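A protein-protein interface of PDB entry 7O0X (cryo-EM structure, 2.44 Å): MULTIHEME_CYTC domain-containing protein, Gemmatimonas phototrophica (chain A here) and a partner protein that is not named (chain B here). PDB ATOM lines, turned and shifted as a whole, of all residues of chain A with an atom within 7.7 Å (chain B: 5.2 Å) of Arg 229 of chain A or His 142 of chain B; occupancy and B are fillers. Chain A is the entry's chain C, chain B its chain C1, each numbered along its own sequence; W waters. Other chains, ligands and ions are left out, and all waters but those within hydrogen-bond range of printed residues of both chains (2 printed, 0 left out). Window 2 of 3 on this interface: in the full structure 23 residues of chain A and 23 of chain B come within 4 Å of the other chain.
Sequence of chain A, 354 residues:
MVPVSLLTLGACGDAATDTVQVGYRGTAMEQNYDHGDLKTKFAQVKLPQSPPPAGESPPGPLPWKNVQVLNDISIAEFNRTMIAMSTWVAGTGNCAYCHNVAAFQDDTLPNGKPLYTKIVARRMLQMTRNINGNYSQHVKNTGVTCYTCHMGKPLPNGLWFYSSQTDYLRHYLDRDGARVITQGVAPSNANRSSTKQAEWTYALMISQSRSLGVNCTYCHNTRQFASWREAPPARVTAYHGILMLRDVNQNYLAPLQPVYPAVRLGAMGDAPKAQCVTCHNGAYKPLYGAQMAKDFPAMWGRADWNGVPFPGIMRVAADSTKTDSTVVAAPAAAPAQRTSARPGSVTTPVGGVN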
ATOM      1  N   GLN A 183     -20.960   8.861 -34.177  1.00  0.00           N
ATOM      2  CA  GLN A 183     -20.240   9.900 -33.439  1.00  0.00           C
ATOM      3  C   GLN A 183     -19.026  10.410 -34.214  1.00  0.00           C
ATOM      4  O   GLN A 183     -17.944  10.608 -33.656  1.00  0.00           O
ATOM      5  CB  GLN A 183     -19.850   9.394 -32.052  1.00  0.00           C
ATOM      6  CG  GLN A 183     -19.611  10.522 -31.044  1.00  0.00           C
ATOM      7  CD  GLN A 183     -19.029  10.049 -29.726  1.00  0.00           C
ATOM      8  OE1 GLN A 183     -17.906   9.551 -29.671  1.00  0.00           O
ATOM      9  NE2 GLN A 183     -19.788  10.221 -28.652  1.00  0.00           N
ATOM     10  N   ASN A 221     -32.022  17.854 -26.934  1.00  0.00           N
ATOM     11  CA  ASN A 221     -32.079  18.898 -27.948  1.00  0.00           C
ATOM     12  C   ASN A 221     -32.140  18.156 -29.277  1.00  0.00           C
ATOM     13  O   ASN A 221     -31.155  17.538 -29.692  1.00  0.00           O
ATOM     14  CB  ASN A 221     -30.872  19.829 -27.861  1.00  0.00           C
ATOM     15  CG  ASN A 221     -30.992  21.037 -28.774  1.00  0.00           C
ATOM     16  OD1 ASN A 221     -31.682  21.003 -29.789  1.00  0.00           O
ATOM     17  ND2 ASN A 221     -30.317  22.118 -28.409  1.00  0.00           N
ATOM     18  N   ARG A 223     -31.967  18.822 -32.308  1.00  0.00           N
ATOM     19  CA  ARG A 223     -30.984  19.050 -33.361  1.00  0.00           C
ATOM     20  C   ARG A 223     -29.863  18.018 -33.323  1.00  0.00           C
ATOM     21  O   ARG A 223     -29.244  17.739 -34.355  1.00  0.00           O
ATOM     22  CB  ARG A 223     -30.419  20.468 -33.275  1.00  0.00           C
ATOM     23  CG  ARG A 223     -29.279  20.659 -32.301  1.00  0.00           C
ATOM     24  CD  ARG A 223     -28.801  22.096 -32.342  1.00  0.00           C
ATOM     25  NE  ARG A 223     -27.645  22.325 -31.486  1.00  0.00           N
ATOM     26  CZ  ARG A 223     -26.905  23.424 -31.511  1.00  0.00           C
ATOM     27  NH1 ARG A 223     -27.212  24.445 -32.290  1.00  0.00           N
ATOM     28  NH2 ARG A 223     -25.841  23.506 -30.719  1.00  0.00           N
ATOM     29  N   GLN A 224     -29.583  17.443 -32.151  1.00  0.00           N
ATOM     30  CA  GLN A 224     -28.675  16.298 -32.048  1.00  0.00           C
ATOM     31  C   GLN A 224     -29.161  15.402 -30.906  1.00  0.00           C
ATOM     32  O   GLN A 224     -28.837  15.638 -29.740  1.00  0.00           O
ATOM     33  CB  GLN A 224     -27.237  16.751 -31.839  1.00  0.00           C
ATOM     34  CG  GLN A 224     -26.190  15.637 -31.806  1.00  0.00           C
ATOM     35  CD  GLN A 224     -26.012  14.878 -33.118  1.00  0.00           C
ATOM     36  OE1 GLN A 224     -25.233  13.929 -33.179  1.00  0.00           O
ATOM     37  NE2 GLN A 224     -26.704  15.302 -34.168  1.00  0.00           N
ATOM     38  N   ALA A 226     -28.215  12.504 -30.109  1.00  0.00           N
ATOM     39  CA  ALA A 226     -27.094  11.858 -29.432  1.00  0.00           C
ATOM     40  C   ALA A 226     -26.365  12.747 -28.429  1.00  0.00           C
ATOM     41  O   ALA A 226     -25.554  12.224 -27.657  1.00  0.00           O
ATOM     42  CB  ALA A 226     -26.095  11.339 -30.466  1.00  0.00           C
ATOM     43  N   SER A 227     -26.613  14.054 -28.407  1.00  0.00           N
ATOM     44  CA  SER A 227     -25.867  14.937 -27.519  1.00  0.00           C
ATOM     45  C   SER A 227     -26.349  14.796 -26.080  1.00  0.00           C
ATOM     46  O   SER A 227     -27.551  14.853 -25.809  1.00  0.00           O
ATOM     47  CB  SER A 227     -25.999  16.388 -27.976  1.00  0.00           C
ATOM     48  OG  SER A 227     -25.237  17.248 -27.152  1.00  0.00           O
ATOM     49  N   TRP A 228     -25.405  14.602 -25.157  1.00  0.00           N
ATOM     50  CA  TRP A 228     -25.685  14.693 -23.729  1.00  0.00           C
ATOM     51  C   TRP A 228     -25.477  16.093 -23.170  1.00  0.00           C
ATOM     52  O   TRP A 228     -26.189  16.494 -22.241  1.00  0.00           O
ATOM     53  CB  TRP A 228     -24.812  13.700 -22.958  1.00  0.00           C
ATOM     54  CG  TRP A 228     -25.158  12.279 -23.253  1.00  0.00           C
ATOM     55  CD1 TRP A 228     -24.651  11.510 -24.257  1.00  0.00           C
ATOM     56  CD2 TRP A 228     -26.119  11.464 -22.572  1.00  0.00           C
ATOM     57  NE1 TRP A 228     -25.217  10.262 -24.230  1.00  0.00           N
ATOM     58  CE2 TRP A 228     -26.124  10.208 -23.206  1.00  0.00           C
ATOM     59  CE3 TRP A 228     -26.967  11.671 -21.480  1.00  0.00           C
ATOM     60  CZ2 TRP A 228     -26.944   9.164 -22.787  1.00  0.00           C
ATOM     61  CZ3 TRP A 228     -27.778  10.632 -21.065  1.00  0.00           C
ATOM     62  CH2 TRP A 228     -27.762   9.396 -21.718  1.00  0.00           C
ATOM     63  N   ARG A 229     -24.510  16.841 -23.707  1.00  0.00           N
ATOM     64  CA  ARG A 229     -24.270  18.209 -23.252  1.00  0.00           C
ATOM     65  C   ARG A 229     -25.443  19.129 -23.569  1.00  0.00           C
ATOM     66  O   ARG A 229     -25.814  19.974 -22.748  1.00  0.00           O
ATOM     67  CB  ARG A 229     -22.984  18.751 -23.880  1.00  0.00           C
ATOM     68  CG  ARG A 229     -22.651  20.169 -23.447  1.00  0.00           C
ATOM     69  CD  ARG A 229     -21.270  20.612 -23.901  1.00  0.00           C
ATOM     70  NE  ARG A 229     -21.185  20.773 -25.347  1.00  0.00           N
ATOM     71  CZ  ARG A 229     -20.204  21.407 -25.975  1.00  0.00           C
ATOM     72  NH1 ARG A 229     -19.155  21.877 -25.322  1.00  0.00           N
ATOM     73  NH2 ARG A 229     -20.262  21.546 -27.296  1.00  0.00           N
ATOM     74  N   GLU A 230     -26.034  18.988 -24.753  1.00  0.00           N
ATOM     75  CA  GLU A 230     -27.163  19.824 -25.138  1.00  0.00           C
ATOM     76  C   GLU A 230     -28.484  19.368 -24.527  1.00  0.00           C
ATOM     77  O   GLU A 230     -29.450  20.136 -24.541  1.00  0.00           O
ATOM     78  CB  GLU A 230     -27.267  19.868 -26.664  1.00  0.00           C
ATOM     79  CG  GLU A 230     -26.048  20.497 -27.322  1.00  0.00           C
ATOM     80  CD  GLU A 230     -26.202  20.695 -28.815  1.00  0.00           C
ATOM     81  OE1 GLU A 230     -27.303  20.444 -29.347  1.00  0.00           O
ATOM     82  OE2 GLU A 230     -25.217  21.107 -29.460  1.00  0.00           O
ATOM     83  N   ALA A 231     -28.551  18.146 -24.007  1.00  0.00           N
ATOM     84  CA  ALA A 231     -29.766  17.597 -23.425  1.00  0.00           C
ATOM     85  C   ALA A 231     -29.964  18.081 -21.988  1.00  0.00           C
ATOM     86  O   ALA A 231     -28.992  18.347 -21.277  1.00  0.00           O
ATOM     87  CB  ALA A 231     -29.710  16.075 -23.446  1.00  0.00           C
ATOM     88  N   PRO A 232     -31.210  18.203 -21.536  1.00  0.00           N
ATOM     89  CA  PRO A 232     -31.468  18.410 -20.105  1.00  0.00           C
ATOM     90  C   PRO A 232     -30.919  17.262 -19.276  1.00  0.00           C
ATOM     91  O   PRO A 232     -30.736  16.146 -19.784  1.00  0.00           O
ATOM     92  CB  PRO A 232     -33.004  18.479 -20.029  1.00  0.00           C
ATOM     93  CG  PRO A 232     -33.420  18.856 -21.419  1.00  0.00           C
ATOM     94  CD  PRO A 232     -32.471  18.081 -22.279  1.00  0.00           C
ATOM     95  N   PRO A 233     -30.647  17.497 -17.990  1.00  0.00           N
ATOM     96  CA  PRO A 233     -30.137  16.419 -17.124  1.00  0.00           C
ATOM     97  C   PRO A 233     -31.081  15.240 -16.953  1.00  0.00           C
ATOM     98  O   PRO A 233     -30.620  14.153 -16.585  1.00  0.00           O
ATOM     99  CB  PRO A 233     -29.898  17.136 -15.787  1.00  0.00           C
ATOM    100  CG  PRO A 233     -29.657  18.554 -16.173  1.00  0.00           C
ATOM    101  CD  PRO A 233     -30.622  18.795 -17.303  1.00  0.00           C
ATOM    102  N   ARG A 235     -32.233  13.342 -19.093  1.00  0.00           N
ATOM    103  CA  ARG A 235     -31.768  12.224 -19.911  1.00  0.00           C
ATOM    104  C   ARG A 235     -30.890  11.254 -19.125  1.00  0.00           C
ATOM    105  O   ARG A 235     -30.951  10.039 -19.347  1.00  0.00           O
ATOM    106  CB  ARG A 235     -31.024  12.737 -21.142  1.00  0.00           C
ATOM    107  CG  ARG A 235     -30.976  11.709 -22.256  1.00  0.00           C
ATOM    108  CD  ARG A 235     -30.134  12.155 -23.430  1.00  0.00           C
ATOM    109  NE  ARG A 235     -30.075  11.110 -24.442  1.00  0.00           N
ATOM    110  CZ  ARG A 235     -29.052  10.906 -25.257  1.00  0.00           C
ATOM    111  NH1 ARG A 235     -28.104  11.813 -25.415  1.00  0.00           N
ATOM    112  NH2 ARG A 235     -29.012   9.792 -25.981  1.00  0.00           N
ATOM    113  N   TYR B 133     -18.265  26.801 -31.158  1.00  0.00           N
ATOM    114  CA  TYR B 133     -17.656  25.472 -31.100  1.00  0.00           C
ATOM    115  C   TYR B 133     -16.358  25.403 -31.897  1.00  0.00           C
ATOM    116  O   TYR B 133     -16.362  25.702 -33.098  1.00  0.00           O
ATOM    117  CB  TYR B 133     -18.638  24.426 -31.623  1.00  0.00           C
ATOM    118  CG  TYR B 133     -19.924  24.301 -30.832  1.00  0.00           C
ATOM    119  CD1 TYR B 133     -19.961  24.570 -29.470  1.00  0.00           C
ATOM    120  CD2 TYR B 133     -21.104  23.911 -31.453  1.00  0.00           C
ATOM    121  CE1 TYR B 133     -21.135  24.438 -28.748  1.00  0.00           C
ATOM    122  CE2 TYR B 133     -22.282  23.790 -30.743  1.00  0.00           C
ATOM    123  CZ  TYR B 133     -22.292  24.051 -29.390  1.00  0.00           C
ATOM    124  OH  TYR B 133     -23.469  23.947 -28.685  1.00  0.00           O
ATOM    125  N   ASP B 138     -13.630  18.798 -30.285  1.00  0.00           N
ATOM    126  CA  ASP B 138     -13.973  19.446 -29.023  1.00  0.00           C
ATOM    127  C   ASP B 138     -15.418  19.179 -28.612  1.00  0.00           C
ATOM    128  O   ASP B 138     -15.691  18.889 -27.442  1.00  0.00           O
ATOM    129  CB  ASP B 138     -13.716  20.949 -29.136  1.00  0.00           C
ATOM    130  CG  ASP B 138     -13.846  21.665 -27.810  1.00  0.00           C
ATOM    131  OD1 ASP B 138     -14.987  21.953 -27.398  1.00  0.00           O
ATOM    132  OD2 ASP B 138     -12.804  21.944 -27.180  1.00  0.00           O
ATOM    133  N   VAL B 139     -16.354  19.275 -29.558  1.00  0.00           N
ATOM    134  CA  VAL B 139     -17.743  18.897 -29.299  1.00  0.00           C
ATOM    135  C   VAL B 139     -17.848  17.444 -28.845  1.00  0.00           C
ATOM    136  O   VAL B 139     -18.564  17.130 -27.887  1.00  0.00           O
ATOM    137  CB  VAL B 139     -18.604  19.167 -30.548  1.00  0.00           C
ATOM    138  CG1 VAL B 139     -19.985  18.548 -30.398  1.00  0.00           C
ATOM    139  CG2 VAL B 139     -18.714  20.661 -30.798  1.00  0.00           C
ATOM    140  N   VAL B 140     -17.134  16.541 -29.517  1.00  0.00           N
ATOM    141  CA  VAL B 140     -17.176  15.123 -29.161  1.00  0.00           C
ATOM    142  C   VAL B 140     -16.503  14.863 -27.815  1.00  0.00           C
ATOM    143  O   VAL B 140     -16.942  13.996 -27.049  1.00  0.00           O
ATOM    144  CB  VAL B 140     -16.547  14.283 -30.287  1.00  0.00           C
ATOM    145  CG1 VAL B 140     -16.387  12.835 -29.861  1.00  0.00           C
ATOM    146  CG2 VAL B 140     -17.398  14.366 -31.542  1.00  0.00           C
ATOM    147  N   ALA B 141     -15.444  15.610 -27.495  1.00  0.00           N
ATOM    148  CA  ALA B 141     -14.804  15.470 -26.188  1.00  0.00           C
ATOM    149  C   ALA B 141     -15.757  15.737 -25.025  1.00  0.00           C
ATOM    150  O   ALA B 141     -15.559  15.195 -23.933  1.00  0.00           O
ATOM    151  CB  ALA B 141     -13.600  16.405 -26.096  1.00  0.00           C
ATOM    152  N   HIS B 142     -16.784  16.561 -25.226  1.00  0.00           N
ATOM    153  CA  HIS B 142     -17.774  16.795 -24.179  1.00  0.00           C
ATOM    154  C   HIS B 142     -18.852  15.720 -24.090  1.00  0.00           C
ATOM    155  O   HIS B 142     -19.573  15.682 -23.088  1.00  0.00           O
ATOM    156  CB  HIS B 142     -18.443  18.159 -24.373  1.00  0.00           C
ATOM    157  CG  HIS B 142     -17.550  19.320 -24.065  1.00  0.00           C
ATOM    158  ND1 HIS B 142     -16.623  19.809 -24.960  1.00  0.00           N
ATOM    159  CD2 HIS B 142     -17.445  20.089 -22.957  1.00  0.00           C
ATOM    160  CE1 HIS B 142     -15.985  20.830 -24.415  1.00  0.00           C
ATOM    161  NE2 HIS B 142     -16.466  21.020 -23.200  1.00  0.00           N
ATOM    162  N   GLU B 143     -18.993  14.863 -25.094  1.00  0.00           N
ATOM    163  CA  GLU B 143     -20.053  13.867 -25.075  1.00  0.00           C
ATOM    164  C   GLU B 143     -19.586  12.585 -24.384  1.00  0.00           C
ATOM    165  O   GLU B 143     -18.422  12.439 -24.007  1.00  0.00           O
ATOM    166  CB  GLU B 143     -20.517  13.574 -26.502  1.00  0.00           C
ATOM    167  CG  GLU B 143     -21.010  14.802 -27.275  1.00  0.00           C
ATOM    168  CD  GLU B 143     -22.257  15.466 -26.698  1.00  0.00           C
ATOM    169  OE1 GLU B 143     -22.754  15.048 -25.631  1.00  0.00           O
ATOM    170  OE2 GLU B 143     -22.741  16.432 -27.322  1.00  0.00           O
ATOM    171  N   ALA B 144     -20.521  11.652 -24.208  1.00  0.00           N
ATOM    172  CA  ALA B 144     -20.170  10.290 -23.829  1.00  0.00           C
ATOM    173  C   ALA B 144     -19.192   9.677 -24.831  1.00  0.00           C
ATOM    174  O   ALA B 144     -19.020  10.163 -25.952  1.00  0.00           O
ATOM    175  CB  ALA B 144     -21.425   9.424 -23.724  1.00  0.00           C
HETATM  176  O   HOH W   1     -17.209  23.264 -26.966  1.00  0.00           O
HETATM  177  O   HOH W   2     -21.103  18.453 -27.150  1.00  0.00           O
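Among the printed residues, pairs that only touch across the chains: Gln 183 of chain A with Val 140 of chain B (3.6 Å), Trp 228 of chain A with Ala 144 of chain B (3.9 Å), Arg 229 of chain A with Tyr 133 of chain B (3.4 Å) and Arg 229 of chain A with Val 139 of chain B (3.9 Å).
Of the 8 printed residues of chain B, 6 touch a printed residue of chain A.
Printed residues of chain B that touch a printed residue of chain A: Tyr 133, Val 139, Val 140, His 142, Glu 143 and Ala 144.
Along chain B the printed residues that touch a printed residue of chain A span positions 133 to 144.
Printed residues of chain A that touch a printed residue of chain B: Gln 183, Arg 223, Ser 227, Trp 228, Arg 229 and Glu 230.
Among the printed residues, 11 pairs touch across the chains.
Among the printed residues, no Asp or Glu carboxylate lies within 4 Å of a Lys or Arg side-chain nitrogen of the other chain.
The guanidinium group (NH2) of Arg 223 of chain A sits at hydrogen-bond distance from the side-chain hydroxyl (OH) of Tyr 133 of chain B (3.2 Å).
N of Arg 229 of chain A lies within hydrogen-bond range of OE1 of Glu 143 of chain B (3.2 Å).
The side-chain carboxylate of Glu 230 of chain A lies within hydrogen-bond range of the side-chain hydroxyl of Tyr 133 of chain B (3.4 Å).
ND1 of His 142 of chain B sits close to NH1 of Arg 229 of chain A (3.3 Å).
O of Ala 144 of chain B is in hydrogen-bond range of NE2 of Gln 183 of chain A (2.8 Å).
The side-chain hydroxyl (OG) of Ser 227 of chain A sits at hydrogen-bond distance from the side-chain carboxylate (OE2) of Glu 143 of chain B, 2.6 Å away.
The backbone NH (N) of Trp 228 of chain A sits at hydrogen-bond distance from the side-chain carboxylate (OE1) of Glu 143 of chain B, 2.7 Å away.
Gln 224 of chain A touches none of the printed residues of chain B.
Of the printed residues of chain B, Ser 227 of chain A touches Glu 143.
Printed residues of chain B within 4 Å of Trp 228 of chain A: Glu 143 (2.7 Å) and Ala 144 (3.9 Å).
Of chain B, only Tyr 133, Val 139, His 142 and Glu 143 come within 4 Å of Arg 229 of chain A.
Asp 138 of chain B touches none of the printed residues of chain A.
Of the printed residues of chain A, Val 140 of chain B touches Gln 183 (3.6 Å).
No residue of chain A comes within 4 Å of Ala 141 of chain B.
His 142 of chain B touches just one residue of chain A: Arg 229 (3.3 Å).
The nearest residue of chain A that does not touch His 142 of chain B is Trp 228 of chain A (5.6 Å).
Water W2 lies within hydrogen-bond range of OE2 of Glu 143 of chain B (2.6 Å), NE of Arg 229 of chain A (2.9 Å) and O of Val 139 of chain B (3.0 Å).
Water W1 bridges OD1 of Asp 138 of chain B (2.6 Å) and NH1 of Arg 229 of chain A (2.9 Å).
ND1 of His 142 of chain B is in hydrogen-bond range of O of Asp 138 of chain B (2.8 Å).
OG of Ser 227 of chain A sits at hydrogen-bond distance from N of Glu 230 of chain A (3.1 Å).
O of Ser 227 of chain A lies within hydrogen-bond range of NH1 of Arg 235 of chain A.
The backbone NH (N) of Arg 223 of chain A lies close to the side-chain amide oxygen (OD1) of Asn 221 of chain A, at 3.3 Å.
The guanidinium group of Arg 223 of chain A is in salt-bridge range of the side-chain carboxylate of Glu 230 of chain A, at 2.8 Å.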
